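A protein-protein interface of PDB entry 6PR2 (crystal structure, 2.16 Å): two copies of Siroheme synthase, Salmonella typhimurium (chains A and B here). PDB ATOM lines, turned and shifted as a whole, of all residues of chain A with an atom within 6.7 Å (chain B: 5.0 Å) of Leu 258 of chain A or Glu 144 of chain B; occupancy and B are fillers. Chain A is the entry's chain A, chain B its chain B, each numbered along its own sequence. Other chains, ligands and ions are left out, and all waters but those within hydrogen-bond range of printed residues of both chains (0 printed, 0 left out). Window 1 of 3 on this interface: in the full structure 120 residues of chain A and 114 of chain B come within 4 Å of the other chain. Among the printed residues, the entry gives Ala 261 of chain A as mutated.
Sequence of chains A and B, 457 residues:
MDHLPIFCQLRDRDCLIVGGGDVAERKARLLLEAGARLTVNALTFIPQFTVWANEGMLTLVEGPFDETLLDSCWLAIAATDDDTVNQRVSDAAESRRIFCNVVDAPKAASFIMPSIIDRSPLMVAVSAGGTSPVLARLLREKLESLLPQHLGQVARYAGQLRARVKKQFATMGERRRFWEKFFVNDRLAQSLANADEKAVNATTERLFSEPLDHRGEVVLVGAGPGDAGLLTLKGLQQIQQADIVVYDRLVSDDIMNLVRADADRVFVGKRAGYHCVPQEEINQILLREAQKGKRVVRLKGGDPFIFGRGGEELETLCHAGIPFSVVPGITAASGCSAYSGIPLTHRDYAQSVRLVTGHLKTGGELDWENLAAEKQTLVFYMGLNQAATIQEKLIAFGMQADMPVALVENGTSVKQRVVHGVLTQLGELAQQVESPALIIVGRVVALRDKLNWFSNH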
ATOM      1  N   ALA A 228      17.135 -34.998  28.933  1.00  0.00           N
ATOM      2  CA  ALA A 228      16.719 -33.651  29.322  1.00  0.00           C
ATOM      3  C   ALA A 228      15.705 -33.688  30.454  1.00  0.00           C
ATOM      4  O   ALA A 228      15.616 -32.734  31.235  1.00  0.00           O
ATOM      5  CB  ALA A 228      16.129 -32.889  28.125  1.00  0.00           C
ATOM      6  N   GLY A 229      14.940 -34.775  30.570  1.00  0.00           N
ATOM      7  CA  GLY A 229      14.032 -34.869  31.694  1.00  0.00           C
ATOM      8  C   GLY A 229      14.712 -34.975  33.052  1.00  0.00           C
ATOM      9  O   GLY A 229      14.030 -34.829  34.074  1.00  0.00           O
ATOM     10  N   LEU A 231      17.167 -32.941  34.069  1.00  0.00           N
ATOM     11  CA  LEU A 231      17.462 -31.627  34.598  1.00  0.00           C
ATOM     12  C   LEU A 231      16.581 -31.367  35.821  1.00  0.00           C
ATOM     13  O   LEU A 231      15.446 -31.855  35.909  1.00  0.00           O
ATOM     14  CB  LEU A 231      17.222 -30.570  33.514  1.00  0.00           C
ATOM     15  CG  LEU A 231      17.774 -29.155  33.744  1.00  0.00           C
ATOM     16  CD1 LEU A 231      19.272 -29.164  33.932  1.00  0.00           C
ATOM     17  CD2 LEU A 231      17.346 -28.213  32.638  1.00  0.00           C
ATOM     18  N   LEU A 236      16.478 -25.888  35.388  1.00  0.00           N
ATOM     19  CA  LEU A 236      15.701 -25.352  34.264  1.00  0.00           C
ATOM     20  C   LEU A 236      15.421 -23.867  34.452  1.00  0.00           C
ATOM     21  O   LEU A 236      15.461 -23.085  33.485  1.00  0.00           O
ATOM     22  CB  LEU A 236      14.387 -26.121  34.074  1.00  0.00           C
ATOM     23  CG  LEU A 236      13.451 -25.506  33.014  1.00  0.00           C
ATOM     24  CD1 LEU A 236      14.042 -25.625  31.633  1.00  0.00           C
ATOM     25  CD2 LEU A 236      12.024 -26.116  33.035  1.00  0.00           C
ATOM     26  N   ILE A 239      18.684 -21.798  33.496  1.00  0.00           N
ATOM     27  CA  ILE A 239      19.012 -21.669  32.079  1.00  0.00           C
ATOM     28  C   ILE A 239      17.906 -20.997  31.283  1.00  0.00           C
ATOM     29  O   ILE A 239      18.177 -20.457  30.201  1.00  0.00           O
ATOM     30  CB  ILE A 239      19.360 -23.014  31.426  1.00  0.00           C
ATOM     31  CG1 ILE A 239      18.135 -23.895  31.301  1.00  0.00           C
ATOM     32  CG2 ILE A 239      20.448 -23.742  32.230  1.00  0.00           C
ATOM     33  CD1 ILE A 239      18.477 -25.298  30.845  1.00  0.00           C
ATOM     34  N   GLN A 240      16.669 -21.006  31.781  1.00  0.00           N
ATOM     35  CA  GLN A 240      15.610 -20.244  31.127  1.00  0.00           C
ATOM     36  C   GLN A 240      15.759 -18.746  31.337  1.00  0.00           C
ATOM     37  O   GLN A 240      15.098 -17.975  30.641  1.00  0.00           O
ATOM     38  CB  GLN A 240      14.235 -20.694  31.625  1.00  0.00           C
ATOM     39  CG  GLN A 240      13.780 -22.002  31.000  1.00  0.00           C
ATOM     40  CD  GLN A 240      13.023 -21.802  29.693  1.00  0.00           C
ATOM     41  OE1 GLN A 240      13.119 -22.627  28.781  1.00  0.00           O
ATOM     42  NE2 GLN A 240      12.251 -20.713  29.605  1.00  0.00           N
ATOM     43  N   ASP A 253      22.207 -32.552  23.656  1.00  0.00           N
ATOM     44  CA  ASP A 253      21.563 -31.641  22.710  1.00  0.00           C
ATOM     45  C   ASP A 253      20.217 -31.169  23.240  1.00  0.00           C
ATOM     46  O   ASP A 253      19.891 -29.978  23.167  1.00  0.00           O
ATOM     47  CB  ASP A 253      21.378 -32.321  21.348  1.00  0.00           C
ATOM     48  CG  ASP A 253      22.670 -32.403  20.546  1.00  0.00           C
ATOM     49  OD1 ASP A 253      22.768 -33.272  19.652  1.00  0.00           O
ATOM     50  OD2 ASP A 253      23.596 -31.609  20.815  1.00  0.00           O
ATOM     51  N   ASP A 254      19.422 -32.095  23.782  1.00  0.00           N
ATOM     52  CA  ASP A 254      18.085 -31.730  24.237  1.00  0.00           C
ATOM     53  C   ASP A 254      18.133 -30.738  25.388  1.00  0.00           C
ATOM     54  O   ASP A 254      17.205 -29.940  25.548  1.00  0.00           O
ATOM     55  CB  ASP A 254      17.301 -32.980  24.630  1.00  0.00           C
ATOM     56  CG  ASP A 254      17.203 -33.976  23.494  1.00  0.00           C
ATOM     57  OD1 ASP A 254      18.113 -34.826  23.376  1.00  0.00           O
ATOM     58  OD2 ASP A 254      16.236 -33.888  22.705  1.00  0.00           O
ATOM     59  N   ILE A 255      19.204 -30.752  26.187  1.00  0.00           N
ATOM     60  CA  ILE A 255      19.314 -29.757  27.248  1.00  0.00           C
ATOM     61  C   ILE A 255      19.491 -28.364  26.653  1.00  0.00           C
ATOM     62  O   ILE A 255      18.871 -27.390  27.108  1.00  0.00           O
ATOM     63  CB  ILE A 255      20.460 -30.106  28.211  1.00  0.00           C
ATOM     64  CG1 ILE A 255      20.214 -31.452  28.895  1.00  0.00           C
ATOM     65  CG2 ILE A 255      20.620 -28.996  29.253  1.00  0.00           C
ATOM     66  CD1 ILE A 255      19.566 -31.361  30.232  1.00  0.00           C
ATOM     67  N   MET A 256      20.310 -28.246  25.603  1.00  0.00           N
ATOM     68  CA  MET A 256      20.550 -26.924  25.034  1.00  0.00           C
ATOM     69  C   MET A 256      19.282 -26.329  24.424  1.00  0.00           C
ATOM     70  O   MET A 256      19.135 -25.101  24.391  1.00  0.00           O
ATOM     71  CB  MET A 256      21.689 -26.985  24.013  1.00  0.00           C
ATOM     72  CG  MET A 256      23.047 -27.258  24.656  1.00  0.00           C
ATOM     73  SD  MET A 256      23.408 -26.135  26.044  1.00  0.00           S
ATOM     74  CE  MET A 256      23.377 -24.557  25.172  1.00  0.00           C
ATOM     75  N   ASN A 257      18.346 -27.167  23.967  1.00  0.00           N
ATOM     76  CA  ASN A 257      17.077 -26.643  23.460  1.00  0.00           C
ATOM     77  C   ASN A 257      16.249 -25.963  24.547  1.00  0.00           C
ATOM     78  O   ASN A 257      15.339 -25.192  24.221  1.00  0.00           O
ATOM     79  CB  ASN A 257      16.242 -27.755  22.826  1.00  0.00           C
ATOM     80  CG  ASN A 257      16.976 -28.485  21.721  1.00  0.00           C
ATOM     81  OD1 ASN A 257      17.948 -27.980  21.159  1.00  0.00           O
ATOM     82  ND2 ASN A 257      16.514 -29.690  21.405  1.00  0.00           N
ATOM     83  N   LEU A 258      16.534 -26.242  25.822  1.00  0.00           N
ATOM     84  CA  LEU A 258      15.807 -25.635  26.931  1.00  0.00           C
ATOM     85  C   LEU A 258      16.346 -24.267  27.318  1.00  0.00           C
ATOM     86  O   LEU A 258      15.723 -23.589  28.145  1.00  0.00           O
ATOM     87  CB  LEU A 258      15.846 -26.544  28.159  1.00  0.00           C
ATOM     88  CG  LEU A 258      15.217 -27.907  27.929  1.00  0.00           C
ATOM     89  CD1 LEU A 258      15.190 -28.698  29.226  1.00  0.00           C
ATOM     90  CD2 LEU A 258      13.831 -27.700  27.363  1.00  0.00           C
ATOM     91  N   VAL A 259      17.495 -23.863  26.775  1.00  0.00           N
ATOM     92  CA  VAL A 259      18.003 -22.531  27.051  1.00  0.00           C
ATOM     93  C   VAL A 259      17.080 -21.505  26.405  1.00  0.00           C
ATOM     94  O   VAL A 259      16.516 -21.740  25.321  1.00  0.00           O
ATOM     95  CB  VAL A 259      19.453 -22.407  26.554  1.00  0.00           C
ATOM     96  CG1 VAL A 259      20.094 -21.150  27.092  1.00  0.00           C
ATOM     97  CG2 VAL A 259      20.253 -23.617  27.013  1.00  0.00           C
ATOM     98  N   ARG A 260      16.879 -20.376  27.082  1.00  0.00           N
ATOM     99  CA  ARG A 260      16.035 -19.357  26.475  1.00  0.00           C
ATOM    100  C   ARG A 260      16.628 -18.939  25.141  1.00  0.00           C
ATOM    101  O   ARG A 260      17.852 -18.902  24.963  1.00  0.00           O
ATOM    102  CB  ARG A 260      15.843 -18.151  27.388  1.00  0.00           C
ATOM    103  CG  ARG A 260      17.030 -17.280  27.612  1.00  0.00           C
ATOM    104  CD  ARG A 260      16.671 -16.334  28.723  1.00  0.00           C
ATOM    105  NE  ARG A 260      17.608 -15.240  28.886  1.00  0.00           N
ATOM    106  CZ  ARG A 260      17.289 -13.965  28.719  1.00  0.00           C
ATOM    107  NH1 ARG A 260      16.054 -13.634  28.377  1.00  0.00           N
ATOM    108  NH2 ARG A 260      18.206 -13.025  28.891  1.00  0.00           N
ATOM    109  N   ALA A 261      15.732 -18.681  24.185  1.00  0.00           N
ATOM    110  CA  ALA A 261      16.144 -18.550  22.797  1.00  0.00           C
ATOM    111  C   ALA A 261      17.072 -17.365  22.601  1.00  0.00           C
ATOM    112  O   ALA A 261      17.938 -17.394  21.719  1.00  0.00           O
ATOM    113  CB  ALA A 261      14.915 -18.423  21.897  1.00  0.00           C
ATOM    114  N   ARG A 265      25.292 -18.217  23.773  1.00  0.00           N
ATOM    115  CA  ARG A 265      25.800 -19.532  24.139  1.00  0.00           C
ATOM    116  C   ARG A 265      27.258 -19.634  23.723  1.00  0.00           C
ATOM    117  O   ARG A 265      27.599 -19.339  22.574  1.00  0.00           O
ATOM    118  CB  ARG A 265      24.975 -20.642  23.483  1.00  0.00           C
ATOM    119  CG  ARG A 265      23.487 -20.410  23.583  1.00  0.00           C
ATOM    120  CD  ARG A 265      22.711 -21.641  23.186  1.00  0.00           C
ATOM    121  NE  ARG A 265      21.282 -21.368  23.077  1.00  0.00           N
ATOM    122  CZ  ARG A 265      20.423 -22.159  22.444  1.00  0.00           C
ATOM    123  NH1 ARG A 265      20.850 -23.277  21.869  1.00  0.00           N
ATOM    124  NH2 ARG A 265      19.135 -21.836  22.399  1.00  0.00           N
ATOM    125  N   ILE B 116       8.302 -19.873  22.416  1.00  0.00           N
ATOM    126  CA  ILE B 116       7.877 -21.120  21.792  1.00  0.00           C
ATOM    127  C   ILE B 116       8.270 -22.299  22.671  1.00  0.00           C
ATOM    128  O   ILE B 116       9.398 -22.355  23.178  1.00  0.00           O
ATOM    129  CB  ILE B 116       8.486 -21.269  20.388  1.00  0.00           C
ATOM    130  CG1 ILE B 116       7.913 -20.213  19.447  1.00  0.00           C
ATOM    131  CG2 ILE B 116       8.267 -22.687  19.855  1.00  0.00           C
ATOM    132  CD1 ILE B 116       8.779 -19.978  18.229  1.00  0.00           C
ATOM    133  N   ILE B 117       7.343 -23.240  22.852  1.00  0.00           N
ATOM    134  CA  ILE B 117       7.656 -24.541  23.441  1.00  0.00           C
ATOM    135  C   ILE B 117       7.454 -25.565  22.332  1.00  0.00           C
ATOM    136  O   ILE B 117       6.326 -25.792  21.877  1.00  0.00           O
ATOM    137  CB  ILE B 117       6.792 -24.873  24.659  1.00  0.00           C
ATOM    138  CG1 ILE B 117       6.984 -23.829  25.745  1.00  0.00           C
ATOM    139  CG2 ILE B 117       7.127 -26.278  25.183  1.00  0.00           C
ATOM    140  CD1 ILE B 117       5.903 -22.764  25.750  1.00  0.00           C
ATOM    141  N   ASP B 118       8.546 -26.188  21.915  1.00  0.00           N
ATOM    142  CA  ASP B 118       8.611 -27.009  20.715  1.00  0.00           C
ATOM    143  C   ASP B 118       8.569 -28.473  21.139  1.00  0.00           C
ATOM    144  O   ASP B 118       9.498 -28.969  21.791  1.00  0.00           O
ATOM    145  CB  ASP B 118       9.892 -26.665  19.950  1.00  0.00           C
ATOM    146  CG  ASP B 118      10.139 -27.557  18.745  1.00  0.00           C
ATOM    147  OD1 ASP B 118       9.261 -28.361  18.369  1.00  0.00           O
ATOM    148  OD2 ASP B 118      11.242 -27.441  18.172  1.00  0.00           O
ATOM    149  N   ARG B 119       7.482 -29.155  20.791  1.00  0.00           N
ATOM    150  CA  ARG B 119       7.362 -30.602  20.919  1.00  0.00           C
ATOM    151  C   ARG B 119       6.873 -31.178  19.598  1.00  0.00           C
ATOM    152  O   ARG B 119       5.983 -32.036  19.557  1.00  0.00           O
ATOM    153  CB  ARG B 119       6.429 -31.006  22.069  1.00  0.00           C
ATOM    154  CG  ARG B 119       6.875 -30.525  23.462  1.00  0.00           C
ATOM    155  CD  ARG B 119       8.152 -31.243  23.948  1.00  0.00           C
ATOM    156  NE  ARG B 119       8.459 -30.877  25.325  1.00  0.00           N
ATOM    157  CZ  ARG B 119       9.125 -29.782  25.681  1.00  0.00           C
ATOM    158  NH1 ARG B 119       9.605 -28.968  24.752  1.00  0.00           N
ATOM    159  NH2 ARG B 119       9.339 -29.516  26.970  1.00  0.00           N
ATOM    160  N   ARG B 140       6.753 -19.694  29.699  1.00  0.00           N
ATOM    161  CA  ARG B 140       7.418 -20.700  28.884  1.00  0.00           C
ATOM    162  C   ARG B 140       8.154 -21.691  29.776  1.00  0.00           C
ATOM    163  O   ARG B 140       8.091 -22.906  29.554  1.00  0.00           O
ATOM    164  CB  ARG B 140       8.387 -20.042  27.892  1.00  0.00           C
ATOM    165  CG  ARG B 140       9.103 -21.043  27.006  1.00  0.00           C
ATOM    166  CD  ARG B 140      10.287 -20.462  26.233  1.00  0.00           C
ATOM    167  NE  ARG B 140      10.899 -21.515  25.420  1.00  0.00           N
ATOM    168  CZ  ARG B 140      12.157 -21.922  25.546  1.00  0.00           C
ATOM    169  NH1 ARG B 140      12.958 -21.341  26.419  1.00  0.00           N
ATOM    170  NH2 ARG B 140      12.627 -22.891  24.781  1.00  0.00           N
ATOM    171  N   GLU B 141       8.801 -21.179  30.826  1.00  0.00           N
ATOM    172  CA  GLU B 141       9.519 -22.023  31.770  1.00  0.00           C
ATOM    173  C   GLU B 141       8.593 -23.048  32.423  1.00  0.00           C
ATOM    174  O   GLU B 141       8.939 -24.233  32.487  1.00  0.00           O
ATOM    175  CB  GLU B 141      10.208 -21.147  32.822  1.00  0.00           C
ATOM    176  CG  GLU B 141      11.286 -21.854  33.593  1.00  0.00           C
ATOM    177  CD  GLU B 141      10.744 -22.627  34.774  1.00  0.00           C
ATOM    178  OE1 GLU B 141       9.657 -22.277  35.288  1.00  0.00           O
ATOM    179  OE2 GLU B 141      11.397 -23.613  35.166  1.00  0.00           O
ATOM    180  N   LYS B 142       7.410 -22.621  32.906  1.00  0.00           N
ATOM    181  CA  LYS B 142       6.473 -23.585  33.495  1.00  0.00           C
ATOM    182  C   LYS B 142       6.026 -24.629  32.478  1.00  0.00           C
ATOM    183  O   LYS B 142       5.882 -25.808  32.816  1.00  0.00           O
ATOM    184  CB  LYS B 142       5.237 -22.906  34.111  1.00  0.00           C
ATOM    185  CG  LYS B 142       5.468 -22.111  35.404  1.00  0.00           C
ATOM    186  CD  LYS B 142       6.424 -20.955  35.200  1.00  0.00           C
ATOM    187  CE  LYS B 142       7.022 -20.293  36.442  1.00  0.00           C
ATOM    188  NZ  LYS B 142       8.403 -19.822  36.080  1.00  0.00           N
ATOM    189  N   LEU B 143       5.785 -24.216  31.235  1.00  0.00           N
ATOM    190  CA  LEU B 143       5.288 -25.159  30.242  1.00  0.00           C
ATOM    191  C   LEU B 143       6.373 -26.142  29.822  1.00  0.00           C
ATOM    192  O   LEU B 143       6.090 -27.322  29.596  1.00  0.00           O
ATOM    193  CB  LEU B 143       4.742 -24.405  29.032  1.00  0.00           C
ATOM    194  CG  LEU B 143       3.514 -23.565  29.398  1.00  0.00           C
ATOM    195  CD1 LEU B 143       3.216 -22.514  28.341  1.00  0.00           C
ATOM    196  CD2 LEU B 143       2.317 -24.468  29.605  1.00  0.00           C
ATOM    197  N   GLU B 144       7.617 -25.668  29.706  1.00  0.00           N
ATOM    198  CA  GLU B 144       8.722 -26.556  29.377  1.00  0.00           C
ATOM    199  C   GLU B 144       8.863 -27.649  30.430  1.00  0.00           C
ATOM    200  O   GLU B 144       9.086 -28.811  30.091  1.00  0.00           O
ATOM    201  CB  GLU B 144      10.025 -25.764  29.252  1.00  0.00           C
ATOM    202  CG  GLU B 144      10.089 -24.872  28.035  1.00  0.00           C
ATOM    203  CD  GLU B 144      10.443 -25.610  26.742  1.00  0.00           C
ATOM    204  OE1 GLU B 144      10.436 -26.861  26.718  1.00  0.00           O
ATOM    205  OE2 GLU B 144      10.728 -24.922  25.741  1.00  0.00           O
ATOM    206  N   SER B 145       8.679 -27.298  31.707  1.00  0.00           N
ATOM    207  CA  SER B 145       8.804 -28.267  32.795  1.00  0.00           C
ATOM    208  C   SER B 145       7.660 -29.278  32.808  1.00  0.00           C
ATOM    209  O   SER B 145       7.831 -30.397  33.303  1.00  0.00           O
ATOM    210  CB  SER B 145       8.861 -27.547  34.136  1.00  0.00           C
ATOM    211  OG  SER B 145       7.563 -27.276  34.627  1.00  0.00           O
ATOM    212  N   LEU B 146       6.498 -28.902  32.281  1.00  0.00           N
ATOM    213  CA  LEU B 146       5.319 -29.747  32.306  1.00  0.00           C
ATOM    214  C   LEU B 146       5.220 -30.672  31.105  1.00  0.00           C
ATOM    215  O   LEU B 146       4.626 -31.751  31.216  1.00  0.00           O
ATOM    216  CB  LEU B 146       4.057 -28.876  32.370  1.00  0.00           C
ATOM    217  CG  LEU B 146       3.851 -28.109  33.683  1.00  0.00           C
ATOM    218  CD1 LEU B 146       2.477 -27.469  33.730  1.00  0.00           C
ATOM    219  CD2 LEU B 146       4.073 -29.001  34.911  1.00  0.00           C
ATOM    220  N   LEU B 147       5.759 -30.274  29.952  1.00  0.00           N
ATOM    221  CA  LEU B 147       5.519 -31.026  28.728  1.00  0.00           C
ATOM    222  C   LEU B 147       6.654 -32.012  28.515  1.00  0.00           C
ATOM    223  O   LEU B 147       7.804 -31.587  28.339  1.00  0.00           O
ATOM    224  CB  LEU B 147       5.377 -30.096  27.535  1.00  0.00           C
ATOM    225  CG  LEU B 147       3.994 -29.428  27.547  1.00  0.00           C
ATOM    226  CD1 LEU B 147       3.828 -28.564  26.319  1.00  0.00           C
ATOM    227  CD2 LEU B 147       2.886 -30.481  27.583  1.00  0.00           C
ATOM    228  N   GLN B 149       9.558 -34.293  27.234  1.00  0.00           N
ATOM    229  CA  GLN B 149      10.474 -34.051  26.123  1.00  0.00           C
ATOM    230  C   GLN B 149      10.091 -34.802  24.852  1.00  0.00           C
ATOM    231  O   GLN B 149      10.350 -34.311  23.747  1.00  0.00           O
ATOM    232  CB  GLN B 149      11.879 -34.446  26.560  1.00  0.00           C
ATOM    233  CG  GLN B 149      12.436 -33.566  27.663  1.00  0.00           C
ATOM    234  CD  GLN B 149      12.592 -32.123  27.194  1.00  0.00           C
ATOM    235  OE1 GLN B 149      13.223 -31.860  26.169  1.00  0.00           O
ATOM    236  NE2 GLN B 149      12.006 -31.184  27.939  1.00  0.00           N
ATOM    237  N   LEU B 233      12.649 -32.753  36.167  1.00  0.00           N
ATOM    238  CA  LEU B 233      11.496 -32.479  35.313  1.00  0.00           C
ATOM    239  C   LEU B 233      10.628 -33.730  35.157  1.00  0.00           C
ATOM    240  O   LEU B 233       9.394 -33.679  35.300  1.00  0.00           O
ATOM    241  CB  LEU B 233      11.963 -31.983  33.940  1.00  0.00           C
ATOM    242  CG  LEU B 233      12.317 -30.508  33.656  1.00  0.00           C
ATOM    243  CD1 LEU B 233      12.984 -29.822  34.825  1.00  0.00           C
ATOM    244  CD2 LEU B 233      13.186 -30.377  32.394  1.00  0.00           C
ATOM    245  N   GLN B 237       6.775 -34.451  36.325  1.00  0.00           N
ATOM    246  CA  GLN B 237       5.758 -34.907  35.387  1.00  0.00           C
ATOM    247  C   GLN B 237       5.095 -36.199  35.871  1.00  0.00           C
ATOM    248  O   GLN B 237       3.879 -36.380  35.729  1.00  0.00           O
ATOM    249  CB  GLN B 237       6.386 -35.097  34.006  1.00  0.00           C
ATOM    250  CG  GLN B 237       6.794 -33.785  33.309  1.00  0.00           C
ATOM    251  CD  GLN B 237       7.954 -33.992  32.349  1.00  0.00           C
ATOM    252  OE1 GLN B 237       8.255 -35.121  31.951  1.00  0.00           O
ATOM    253  NE2 GLN B 237       8.638 -32.916  32.011  1.00  0.00           N
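Among the printed residues, merely in contact across the chains: Ala 228 of chain A with Gln 149 of chain B, Ala 228 of chain A with Leu 233 of chain B, Leu 236 of chain A with Glu 141 of chain B, Leu 236 of chain A with Ser 145 of chain B, Gln 240 of chain A with Glu 141 of chain B, Gln 240 of chain A with Glu 144 of chain B, Asn 257 of chain A with Arg 140 of chain B, Leu 258 of chain A with Arg 140 of chain B, Leu 258 of chain A with Glu 144 of chain B, Leu 258 of chain A with Gln 149 of chain B, Val 259 of chain A with Arg 140 of chain B and Arg 260 of chain A with Arg 140 of chain B.
The side-chain amide oxygen (OE1) of Gln 240 of chain A is in hydrogen-bond range of the guanidinium group (NH1) of Arg 140 of chain B (2.7 Å).
The backbone carbonyl oxygen (O) of Gly 229 of chain A lies within hydrogen-bond range of the backbone NH (N) of Leu 233 of chain B.
The backbone carbonyl oxygen (O) of Leu 231 of chain A is in hydrogen-bond range of the backbone NH (N) of Leu 233 of chain B (2.9 Å).
No position is printed for both chains.
Of the 15 pairs that touch across the chains among the printed residues, none has its exchanged pair printed and touching as well.
Of the 16 printed residues of chain A, 9 touch a printed residue of chain B.
Hydrophobic or aromatic side chains of chain A that line the printed part of chain B: Ala 228, Leu 236 and Leu 258.
Among the printed residues, no Asp or Glu carboxylate lies within 4 Å of a Lys or Arg side-chain nitrogen of the other chain.
Glu 144 of chain B touches just these residues of chain A: Gln 240 and Leu 258.
Printed residues of chain B within 4 Å of Gly 229 of chain A: Leu 233.
Of the printed residues of chain A, Gln 149 of chain B touches Ala 228 and Leu 258.
Of the printed residues of chain A, Ser 145 of chain B touches Leu 236.
Ile 117 of chain B touches none of the printed residues of chain A.
Asp 118 of chain B touches none of the printed residues of chain A.
OE1 of Glu 141 of chain B is in salt-bridge range of NZ of Lys 142 of chain B (2.9 Å).
The side-chain hydroxyl (OG) of Ser 145 of chain B sits at hydrogen-bond distance from the backbone carbonyl oxygen (O) of Lys 142 of chain B, at 2.9 Å.
O of Asp 253 of chain A lies close to OD1 of Asn 257 of chain A (3.4 Å).
The side-chain amide nitrogen of Gln 149 of chain B lies close to the guanidinium group of Arg 119 of chain B (3.3 Å).
The backbone carbonyl oxygen of Leu 233 of chain B sits close to the side-chain amide nitrogen of Gln 237 of chain B.
The backbone carbonyl oxygen of Ser 145 of chain B lies within hydrogen-bond range of the side-chain amide nitrogen of Gln 237 of chain B.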
